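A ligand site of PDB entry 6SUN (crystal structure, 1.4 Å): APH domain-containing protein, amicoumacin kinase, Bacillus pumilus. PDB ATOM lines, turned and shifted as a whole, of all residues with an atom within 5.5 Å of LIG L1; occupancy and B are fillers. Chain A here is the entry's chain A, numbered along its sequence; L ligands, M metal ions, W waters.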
ATOM      1  N   GLU A  36      -3.531  28.225   4.086  1.00  0.00           N
ATOM      2  CA  GLU A  36      -2.748  27.513   5.100  1.00  0.00           C
ATOM      3  C   GLU A  36      -2.840  28.204   6.480  1.00  0.00           C
ATOM      4  O   GLU A  36      -3.191  27.606   7.490  1.00  0.00           O
ATOM      5  CB  GLU A  36      -1.295  27.442   4.606  1.00  0.00           C
ATOM      6  CG  GLU A  36      -0.458  26.330   5.196  1.00  0.00           C
ATOM      7  CD  GLU A  36      -0.653  25.009   4.467  1.00  0.00           C
ATOM      8  OE1 GLU A  36      -1.724  24.396   4.647  1.00  0.00           O
ATOM      9  OE2 GLU A  36       0.263  24.589   3.716  1.00  0.00           O
ATOM     10  N   GLU A 160       7.946  15.053   9.847  1.00  0.00           N
ATOM     11  CA  GLU A 160       7.035  15.829   9.027  1.00  0.00           C
ATOM     12  C   GLU A 160       5.742  15.064   8.774  1.00  0.00           C
ATOM     13  O   GLU A 160       5.763  13.971   8.187  1.00  0.00           O
ATOM     14  CB  GLU A 160       7.707  16.194   7.713  1.00  0.00           C
ATOM     15  CG  GLU A 160       6.809  16.821   6.656  1.00  0.00           C
ATOM     16  CD  GLU A 160       6.073  18.055   7.145  1.00  0.00           C
ATOM     17  OE1 GLU A 160       6.783  19.045   7.493  1.00  0.00           O
ATOM     18  OE2 GLU A 160       4.805  18.078   7.149  1.00  0.00           O
ATOM     19  N   GLN A 162       3.425  15.530   6.697  1.00  0.00           N
ATOM     20  CA  GLN A 162       3.103  15.333   5.301  1.00  0.00           C
ATOM     21  C   GLN A 162       3.883  14.204   4.621  1.00  0.00           C
ATOM     22  O   GLN A 162       3.588  13.862   3.468  1.00  0.00           O
ATOM     23  CB  GLN A 162       3.147  16.679   4.551  1.00  0.00           C
ATOM     24  CG  GLN A 162       2.039  17.585   5.124  1.00  0.00           C
ATOM     25  CD  GLN A 162       1.932  18.965   4.542  1.00  0.00           C
ATOM     26  OE1 GLN A 162       2.923  19.589   4.221  1.00  0.00           O
ATOM     27  NE2 GLN A 162       0.696  19.483   4.484  1.00  0.00           N
ATOM     28  N   ALA A 202      13.860  24.813   4.905  1.00  0.00           N
ATOM     29  CA  ALA A 202      13.109  23.624   4.462  1.00  0.00           C
ATOM     30  C   ALA A 202      11.949  23.866   3.509  1.00  0.00           C
ATOM     31  O   ALA A 202      11.201  22.932   3.179  1.00  0.00           O
ATOM     32  CB  ALA A 202      12.692  22.730   5.637  1.00  0.00           C
ATOM     33  N   ASP A 203      11.788  25.090   3.025  1.00  0.00           N
ATOM     34  CA  ASP A 203      10.751  25.404   2.016  1.00  0.00           C
ATOM     35  C   ASP A 203      11.278  26.532   1.126  1.00  0.00           C
ATOM     36  O   ASP A 203      10.558  27.512   0.847  1.00  0.00           O
ATOM     37  CB  ASP A 203       9.434  25.811   2.713  1.00  0.00           C
ATOM     38  CG  ASP A 203       8.231  25.894   1.757  1.00  0.00           C
ATOM     39  OD1 ASP A 203       8.255  25.232   0.722  1.00  0.00           O
ATOM     40  OD2 ASP A 203       7.260  26.630   2.095  1.00  0.00           O
ATOM     41  N   HIS A 205      12.051  28.443  -2.094  1.00  0.00           N
ATOM     42  CA  HIS A 205      11.609  28.611  -3.458  1.00  0.00           C
ATOM     43  C   HIS A 205      11.295  30.076  -3.645  1.00  0.00           C
ATOM     44  O   HIS A 205      11.230  30.847  -2.694  1.00  0.00           O
ATOM     45  CB  HIS A 205      10.404  27.728  -3.812  1.00  0.00           C
ATOM     46  CG  HIS A 205       9.194  27.946  -2.979  1.00  0.00           C
ATOM     47  ND1 HIS A 205       8.433  29.092  -3.031  1.00  0.00           N
ATOM     48  CD2 HIS A 205       8.640  27.166  -2.025  1.00  0.00           C
ATOM     49  CE1 HIS A 205       7.424  28.988  -2.178  1.00  0.00           C
ATOM     50  NE2 HIS A 205       7.531  27.831  -1.546  1.00  0.00           N
ATOM     51  N   HIS A 206      11.084  30.429  -4.904  1.00  0.00           N
ATOM     52  CA  HIS A 206      10.866  31.822  -5.311  1.00  0.00           C
ATOM     53  C   HIS A 206       9.501  32.408  -5.012  1.00  0.00           C
ATOM     54  O   HIS A 206       9.210  33.561  -5.349  1.00  0.00           O
ATOM     55  CB  HIS A 206      11.288  32.030  -6.774  1.00  0.00           C
ATOM     56  CG  HIS A 206      10.743  31.008  -7.713  1.00  0.00           C
ATOM     57  ND1 HIS A 206      11.163  29.691  -7.735  1.00  0.00           N
ATOM     58  CD2 HIS A 206       9.861  31.143  -8.729  1.00  0.00           C
ATOM     59  CE1 HIS A 206      10.537  29.052  -8.709  1.00  0.00           C
ATOM     60  NE2 HIS A 206       9.744  29.914  -9.331  1.00  0.00           N
ATOM     61  N   GLY A 207       8.631  31.649  -4.388  1.00  0.00           N
ATOM     62  CA  GLY A 207       7.494  32.211  -3.685  1.00  0.00           C
ATOM     63  C   GLY A 207       7.734  32.619  -2.241  1.00  0.00           C
ATOM     64  O   GLY A 207       6.852  33.212  -1.628  1.00  0.00           O
ATOM     65  N   ASN A 208       8.922  32.310  -1.712  1.00  0.00           N
ATOM     66  CA  ASN A 208       9.230  32.495  -0.295  1.00  0.00           C
ATOM     67  C   ASN A 208      10.442  33.417  -0.046  1.00  0.00           C
ATOM     68  O   ASN A 208      11.005  33.431   1.033  1.00  0.00           O
ATOM     69  CB  ASN A 208       9.471  31.170   0.409  1.00  0.00           C
ATOM     70  CG  ASN A 208       8.201  30.467   0.812  1.00  0.00           C
ATOM     71  OD1 ASN A 208       7.092  31.032   0.827  1.00  0.00           O
ATOM     72  ND2 ASN A 208       8.387  29.247   1.295  1.00  0.00           N
ATOM     73  N   ASP A 223       8.006  25.961   7.954  1.00  0.00           N
ATOM     74  CA  ASP A 223       8.359  24.551   7.905  1.00  0.00           C
ATOM     75  C   ASP A 223       9.798  24.264   8.347  1.00  0.00           C
ATOM     76  O   ASP A 223      10.276  23.146   8.190  1.00  0.00           O
ATOM     77  CB  ASP A 223       8.053  24.004   6.522  1.00  0.00           C
ATOM     78  CG  ASP A 223       6.559  23.914   6.268  1.00  0.00           C
ATOM     79  OD1 ASP A 223       5.821  23.373   7.135  1.00  0.00           O
ATOM     80  OD2 ASP A 223       6.110  24.391   5.207  1.00  0.00           O
ATOM     81  N   ASN A 239      11.885  22.740  -6.564  1.00  0.00           N
ATOM     82  CA  ASN A 239      10.968  23.839  -6.777  1.00  0.00           C
ATOM     83  C   ASN A 239      11.282  24.674  -8.009  1.00  0.00           C
ATOM     84  O   ASN A 239      10.371  25.084  -8.712  1.00  0.00           O
ATOM     85  CB  ASN A 239      10.873  24.695  -5.516  1.00  0.00           C
ATOM     86  CG  ASN A 239      10.162  23.964  -4.378  1.00  0.00           C
ATOM     87  OD1 ASN A 239       9.240  23.210  -4.626  1.00  0.00           O
ATOM     88  ND2 ASN A 239      10.550  24.237  -3.139  1.00  0.00           N
ATOM     89  N   VAL A 240      12.567  24.905  -8.284  1.00  0.00           N
ATOM     90  CA  VAL A 240      12.913  25.603  -9.522  1.00  0.00           C
ATOM     91  C   VAL A 240      12.671  24.754 -10.764  1.00  0.00           C
ATOM     92  O   VAL A 240      12.356  25.292 -11.823  1.00  0.00           O
ATOM     93  CB  VAL A 240      14.350  26.182  -9.519  1.00  0.00           C
ATOM     94  CG1 VAL A 240      14.542  27.141  -8.367  1.00  0.00           C
ATOM     95  CG2 VAL A 240      15.424  25.128  -9.546  1.00  0.00           C
ATOM     96  N   TRP A 242      10.133  22.601 -10.916  1.00  0.00           N
ATOM     97  CA  TRP A 242       8.666  22.452 -10.969  1.00  0.00           C
ATOM     98  C   TRP A 242       8.008  23.683 -11.578  1.00  0.00           C
ATOM     99  O   TRP A 242       7.184  23.573 -12.489  1.00  0.00           O
ATOM    100  CB  TRP A 242       8.156  22.168  -9.574  1.00  0.00           C
ATOM    101  CG  TRP A 242       6.718  21.796  -9.449  1.00  0.00           C
ATOM    102  CD1 TRP A 242       5.852  21.469 -10.437  1.00  0.00           C
ATOM    103  CD2 TRP A 242       5.994  21.722  -8.218  1.00  0.00           C
ATOM    104  NE1 TRP A 242       4.612  21.180  -9.891  1.00  0.00           N
ATOM    105  CE2 TRP A 242       4.677  21.320  -8.529  1.00  0.00           C
ATOM    106  CE3 TRP A 242       6.328  21.940  -6.858  1.00  0.00           C
ATOM    107  CZ2 TRP A 242       3.699  21.153  -7.543  1.00  0.00           C
ATOM    108  CZ3 TRP A 242       5.376  21.760  -5.901  1.00  0.00           C
ATOM    109  CH2 TRP A 242       4.062  21.362  -6.236  1.00  0.00           C
ATOM    110  N   TYR A 243       8.385  24.859 -11.057  1.00  0.00           N
ATOM    111  CA  TYR A 243       7.822  26.133 -11.499  1.00  0.00           C
ATOM    112  C   TYR A 243       8.890  27.137 -11.926  1.00  0.00           C
ATOM    113  O   TYR A 243       9.037  28.198 -11.333  1.00  0.00           O
ATOM    114  CB  TYR A 243       6.974  26.731 -10.382  1.00  0.00           C
ATOM    115  CG  TYR A 243       5.691  25.971 -10.109  1.00  0.00           C
ATOM    116  CD1 TYR A 243       4.679  25.910 -11.067  1.00  0.00           C
ATOM    117  CD2 TYR A 243       5.481  25.317  -8.897  1.00  0.00           C
ATOM    118  CE1 TYR A 243       3.496  25.233 -10.829  1.00  0.00           C
ATOM    119  CE2 TYR A 243       4.284  24.678  -8.645  1.00  0.00           C
ATOM    120  CZ  TYR A 243       3.318  24.611  -9.623  1.00  0.00           C
ATOM    121  OH  TYR A 243       2.136  23.951  -9.402  1.00  0.00           O
ATOM    122  N   ARG A 287      10.716  14.514  -1.985  1.00  0.00           N
ATOM    123  CA  ARG A 287       9.882  15.687  -2.144  1.00  0.00           C
ATOM    124  C   ARG A 287       8.707  15.417  -3.090  1.00  0.00           C
ATOM    125  O   ARG A 287       7.569  15.822  -2.820  1.00  0.00           O
ATOM    126  CB  ARG A 287      10.698  16.895  -2.611  1.00  0.00           C
ATOM    127  CG  ARG A 287       9.963  18.235  -2.563  1.00  0.00           C
ATOM    128  CD  ARG A 287       9.390  18.526  -1.167  1.00  0.00           C
ATOM    129  NE  ARG A 287       9.302  19.936  -0.752  1.00  0.00           N
ATOM    130  CZ  ARG A 287       9.413  20.328   0.510  1.00  0.00           C
ATOM    131  NH1 ARG A 287       9.765  19.445   1.486  1.00  0.00           N
ATOM    132  NH2 ARG A 287       9.265  21.610   0.797  1.00  0.00           N
ATOM    133  N   LEU A 290       6.116  13.663  -1.074  1.00  0.00           N
ATOM    134  CA  LEU A 290       5.406  14.601  -0.217  1.00  0.00           C
ATOM    135  C   LEU A 290       4.369  15.389  -1.037  1.00  0.00           C
ATOM    136  O   LEU A 290       3.212  15.532  -0.636  1.00  0.00           O
ATOM    137  CB  LEU A 290       6.403  15.524   0.463  1.00  0.00           C
ATOM    138  CG  LEU A 290       5.863  16.422   1.579  1.00  0.00           C
ATOM    139  CD1 LEU A 290       6.965  16.870   2.530  1.00  0.00           C
ATOM    140  CD2 LEU A 290       5.162  17.644   1.022  1.00  0.00           C
ATOM    141  N   ILE A 291       4.776  15.890  -2.185  1.00  0.00           N
ATOM    142  CA  ILE A 291       3.866  16.656  -3.048  1.00  0.00           C
ATOM    143  C   ILE A 291       2.695  15.786  -3.496  1.00  0.00           C
ATOM    144  O   ILE A 291       1.556  16.274  -3.528  1.00  0.00           O
ATOM    145  CB  ILE A 291       4.601  17.246  -4.278  1.00  0.00           C
ATOM    146  CG1 ILE A 291       5.690  18.229  -3.843  1.00  0.00           C
ATOM    147  CG2 ILE A 291       3.616  17.905  -5.238  1.00  0.00           C
ATOM    148  CD1 ILE A 291       5.221  19.332  -2.964  1.00  0.00           C
ATOM    149  N   LEU A 294       0.193  15.962  -0.891  1.00  0.00           N
ATOM    150  CA  LEU A 294      -0.411  17.312  -0.883  1.00  0.00           C
ATOM    151  C   LEU A 294      -1.455  17.517  -1.964  1.00  0.00           C
ATOM    152  O   LEU A 294      -2.464  18.197  -1.734  1.00  0.00           O
ATOM    153  CB  LEU A 294       0.653  18.390  -1.066  1.00  0.00           C
ATOM    154  CG  LEU A 294       1.510  18.754   0.129  1.00  0.00           C
ATOM    155  CD1 LEU A 294       2.434  19.898  -0.258  1.00  0.00           C
ATOM    156  CD2 LEU A 294       0.657  19.196   1.299  1.00  0.00           C
ATOM    157  N   LEU A 295      -1.219  16.931  -3.127  1.00  0.00           N
ATOM    158  CA  LEU A 295      -2.148  17.038  -4.230  1.00  0.00           C
ATOM    159  C   LEU A 295      -3.465  16.385  -3.894  1.00  0.00           C
ATOM    160  O   LEU A 295      -4.517  16.876  -4.297  1.00  0.00           O
ATOM    161  CB  LEU A 295      -1.578  16.406  -5.496  1.00  0.00           C
ATOM    162  CG  LEU A 295      -0.328  17.086  -6.031  1.00  0.00           C
ATOM    163  CD1 LEU A 295       0.139  16.426  -7.306  1.00  0.00           C
ATOM    164  CD2 LEU A 295      -0.550  18.574  -6.249  1.00  0.00           C
HETATM  165  C1  LIG L   1       5.947  25.284  -4.434  1.00  0.00           C
HETATM  166  C2  LIG L   1       6.529  26.417  -5.236  1.00  0.00           C
HETATM  167  C3  LIG L   1       7.614  26.158  -6.062  1.00  0.00           C
HETATM  168  C4  LIG L   1       8.160  27.219  -6.800  1.00  0.00           C
HETATM  169  C5  LIG L   1       7.632  28.483  -6.662  1.00  0.00           C
HETATM  170  C6  LIG L   1       6.534  28.741  -5.855  1.00  0.00           C
HETATM  171  O1  LIG L   1       6.001  29.981  -5.735  1.00  0.00           O
HETATM  172  C7  LIG L   1       5.993  27.677  -5.126  1.00  0.00           C
HETATM  173  C8  LIG L   1       4.839  27.909  -4.208  1.00  0.00           C
HETATM  174  O2  LIG L   1       4.488  29.017  -3.850  1.00  0.00           O
HETATM  175  O3  LIG L   1       4.225  26.795  -3.607  1.00  0.00           O
HETATM  176  C9  LIG L   1       4.442  25.528  -4.230  1.00  0.00           C
HETATM  177  C10 LIG L   1       3.784  24.478  -3.379  1.00  0.00           C
HETATM  178  C11 LIG L   1       2.275  24.752  -3.283  1.00  0.00           C
HETATM  179  C12 LIG L   1       1.506  23.690  -2.522  1.00  0.00           C
HETATM  180  C13 LIG L   1       0.056  24.154  -2.403  1.00  0.00           C
HETATM  181  C14 LIG L   1       1.603  22.324  -3.162  1.00  0.00           C
HETATM  182  N1  LIG L   1       4.386  24.444  -2.036  1.00  0.00           N
HETATM  183  C15 LIG L   1       5.152  23.444  -1.642  1.00  0.00           C
HETATM  184  O4  LIG L   1       5.378  22.473  -2.353  1.00  0.00           O
HETATM  185  C16 LIG L   1       5.772  23.500  -0.251  1.00  0.00           C
HETATM  186  O5  LIG L   1       5.526  24.727   0.395  1.00  0.00           O
HETATM  187  C17 LIG L   1       5.204  22.371   0.630  1.00  0.00           C
HETATM  188  O6  LIG L   1       5.625  21.148   0.064  1.00  0.00           O
HETATM  189  C18 LIG L   1       5.744  22.412   2.055  1.00  0.00           C
HETATM  190  N2  LIG L   1       5.067  23.459   2.819  1.00  0.00           N
HETATM  191  C19 LIG L   1       5.572  21.054   2.741  1.00  0.00           C
HETATM  192  C20 LIG L   1       6.161  20.999   4.119  1.00  0.00           C
HETATM  193  O7  LIG L   1       7.264  21.453   4.369  1.00  0.00           O
HETATM  194  N3  LIG L   1       5.372  20.472   5.037  1.00  0.00           N
HETATM  195  P1  LG2 L   2       2.137  28.921   1.781  1.00  0.00           P
HETATM  196  O1  LG2 L   2       3.365  28.651   2.591  1.00  0.00           O
HETATM  197  O2  LG2 L   2       1.358  27.726   1.325  1.00  0.00           O
HETATM  198  O3  LG2 L   2       2.571  29.861   0.647  1.00  0.00           O
HETATM  199  P2  LG2 L   2       1.373  30.633   4.152  1.00  0.00           P
HETATM  200  O4  LG2 L   2       0.059  30.806   4.850  1.00  0.00           O
HETATM  201  O5  LG2 L   2       2.475  29.989   4.932  1.00  0.00           O
HETATM  202  N1  LG2 L   2       1.024  29.847   2.688  1.00  0.00           N
HETATM  203  P3  LG2 L   2       3.221  32.811   3.452  1.00  0.00           P
HETATM  204  O6  LG2 L   2       3.964  32.998   4.721  1.00  0.00           O
HETATM  205  O7  LG2 L   2       3.876  32.199   2.285  1.00  0.00           O
HETATM  206  O8  LG2 L   2       1.810  32.141   3.744  1.00  0.00           O
HETATM  207  O9  LG2 L   2       2.669  34.237   3.045  1.00  0.00           O
HETATM  208  C1  LG2 L   2       1.800  34.430   1.920  1.00  0.00           C
HETATM  209  C2  LG2 L   2       2.334  35.547   1.037  1.00  0.00           C
HETATM  210  O10 LG2 L   2       2.467  36.768   1.769  1.00  0.00           O
HETATM  211  C3  LG2 L   2       3.706  35.279   0.415  1.00  0.00           C
HETATM  212  O11 LG2 L   2       3.659  34.441  -0.738  1.00  0.00           O
HETATM  213  C4  LG2 L   2       4.203  36.674   0.140  1.00  0.00           C
HETATM  214  O12 LG2 L   2       3.634  37.183  -1.069  1.00  0.00           O
HETATM  215  C5  LG2 L   2       3.680  37.415   1.332  1.00  0.00           C
HETATM  216  N2  LG2 L   2       4.590  37.442   2.496  1.00  0.00           N
HETATM  217  C6  LG2 L   2       4.616  36.615   3.586  1.00  0.00           C
HETATM  218  N3  LG2 L   2       5.545  36.974   4.453  1.00  0.00           N
HETATM  219  C7  LG2 L   2       6.176  38.023   3.908  1.00  0.00           C
HETATM  220  C8  LG2 L   2       7.204  38.929   4.350  1.00  0.00           C
HETATM  221  N4  LG2 L   2       7.800  38.762   5.510  1.00  0.00           N
HETATM  222  N5  LG2 L   2       7.591  39.918   3.529  1.00  0.00           N
HETATM  223  C9  LG2 L   2       6.984  40.123   2.337  1.00  0.00           C
HETATM  224  N6  LG2 L   2       5.972  39.379   1.883  1.00  0.00           N
HETATM  225  C10 LG2 L   2       5.558  38.326   2.616  1.00  0.00           C
HETATM  226 CA    CA M   1       4.836  30.353   1.289  1.00  0.00          CA
HETATM  227 CA    CA M   2       4.196  28.439   4.700  1.00  0.00          CA
HETATM  228  O   HOH W   1       3.180  31.656  -2.917  1.00  0.00           O
HETATM  229  O   HOH W   2       3.311  26.766  -0.535  1.00  0.00           O
HETATM  230  O   HOH W   3       3.385  22.479   6.674  1.00  0.00           O
HETATM  231  O   HOH W   4       2.172  28.921  -1.988  1.00  0.00           O
HETATM  232  O   HOH W   5       5.468  28.116   0.530  1.00  0.00           O
HETATM  233  O   HOH W   6       2.549  25.329   2.453  1.00  0.00           O
HETATM  234  O   HOH W   7       2.397  22.384   3.343  1.00  0.00           O
HETATM  235  O   HOH W   8       4.519  33.086  -5.297  1.00  0.00           O
HETATM  236  O   HOH W   9       8.145  21.916  -2.497  1.00  0.00           O
HETATM  237  O   HOH W  10       6.068  31.516  -8.024  1.00  0.00           O
HETATM  238  O   HOH W  11       9.881  20.780   4.139  1.00  0.00           O
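An oxygen (O1) of LIG L1 lies close to the backbone NH of Gly 207 (3.4 Å).
The side-chain amide oxygen (OE1) of Gln 162 sits at hydrogen-bond distance from a nitrogen (N3) of LIG L1.
N3 of LIG L1 sits at hydrogen-bond distance from OE1 of Glu 160 (3.2 Å).
OD2 of Asp 203 lies within salt-bridge range of N2 of LIG L1, at 3.9 Å.
The side-chain carboxylate of Asp 223 lies within salt-bridge range of a nitrogen (N2) of LIG L1, at 2.8 Å.
The backbone carbonyl oxygen (O) of Ala 202 lies within hydrogen-bond range of the guanidinium group (NH2) of Arg 287 (3.3 Å).
The guanidinium group (NH2) of Arg 287 lies within salt-bridge range of the side-chain carboxylate (OD1) of Asp 203 (3.8 Å).
NE2 of His 206 is in hydrogen-bond range of O of Tyr 243, 2.7 Å away.
The backbone NH of Gly 207 is in hydrogen-bond range of a ring nitrogen (ND1) of His 205, at 2.9 Å.
OE2 of Glu 160 is in hydrogen-bond range of N of Gln 162 (2.9 Å).
NE2 of His 205 sits at hydrogen-bond distance from ND2 of Asn 208, 3.3 Å away.
The side-chain amide nitrogen of Asn 208 sits at hydrogen-bond distance from the backbone carbonyl oxygen of Asp 203 (2.8 Å).
His 205 touches LIG L1 (CE1 to O2, 3.4 Å).
CE1 of His 206 touches C4 of LIG L1, 3.6 Å away.
Asn 239 touches LIG L1 (CB to C3, 3.6 Å).
CZ3 of Trp 242 touches O4 of LIG L1, 3.6 Å away.
CD2 of Tyr 243 touches C3 of LIG L1 (3.6 Å).
NH2 of Arg 287 touches O6 of LIG L1, at 3.7 Å.
CD2 of Leu 290 touches O6 of LIG L1, 3.7 Å away.
Ile 291 touches LIG L1.
Leu 294 touches LIG L1.
Hydrophobic or aromatic side chains that line LIG L1: His 205, His 206, Trp 242, Tyr 243, Leu 290, Ile 291 and Leu 294.
Of the 19 residues printed, 14 come within 4 Å of LIG L1.
The nearest printed residue that does not touch LIG L1 is Ala 202 (4.4 Å).
Water W11 lies within hydrogen-bond range of the backbone carbonyl oxygen (O) of Ala 202, an oxygen (O7) of LIG L1 and the guanidinium group (NH1) of Arg 287.
Water W9 lies within hydrogen-bond range of OD1 of Asn 239 (2.7 Å), O4 of LIG L1 (2.8 Å) and NE of Arg 287 (2.9 Å).
Water W2 lies within hydrogen-bond range of O2 of LG2 L2 (2.9 Å) and N1 of LIG L1 (3.0 Å).
Water W6 lies within hydrogen-bond range of OE2 of Glu 36 (2.7 Å), O2 of LG2 L2 (2.9 Å) and N2 of LIG L1 (3.2 Å).
Water W3 bridges OD1 of Asp 223 (2.6 Å) and N3 of LIG L1 (3.3 Å).
Water W5 lies within hydrogen-bond range of the side-chain carboxylate of Asp 203 (2.8 Å), a ring nitrogen (NE2) of His 205 (2.9 Å), the side-chain amide nitrogen of Asn 208 (3.2 Å) and an oxygen (O5) of LIG L1 (3.4 Å).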
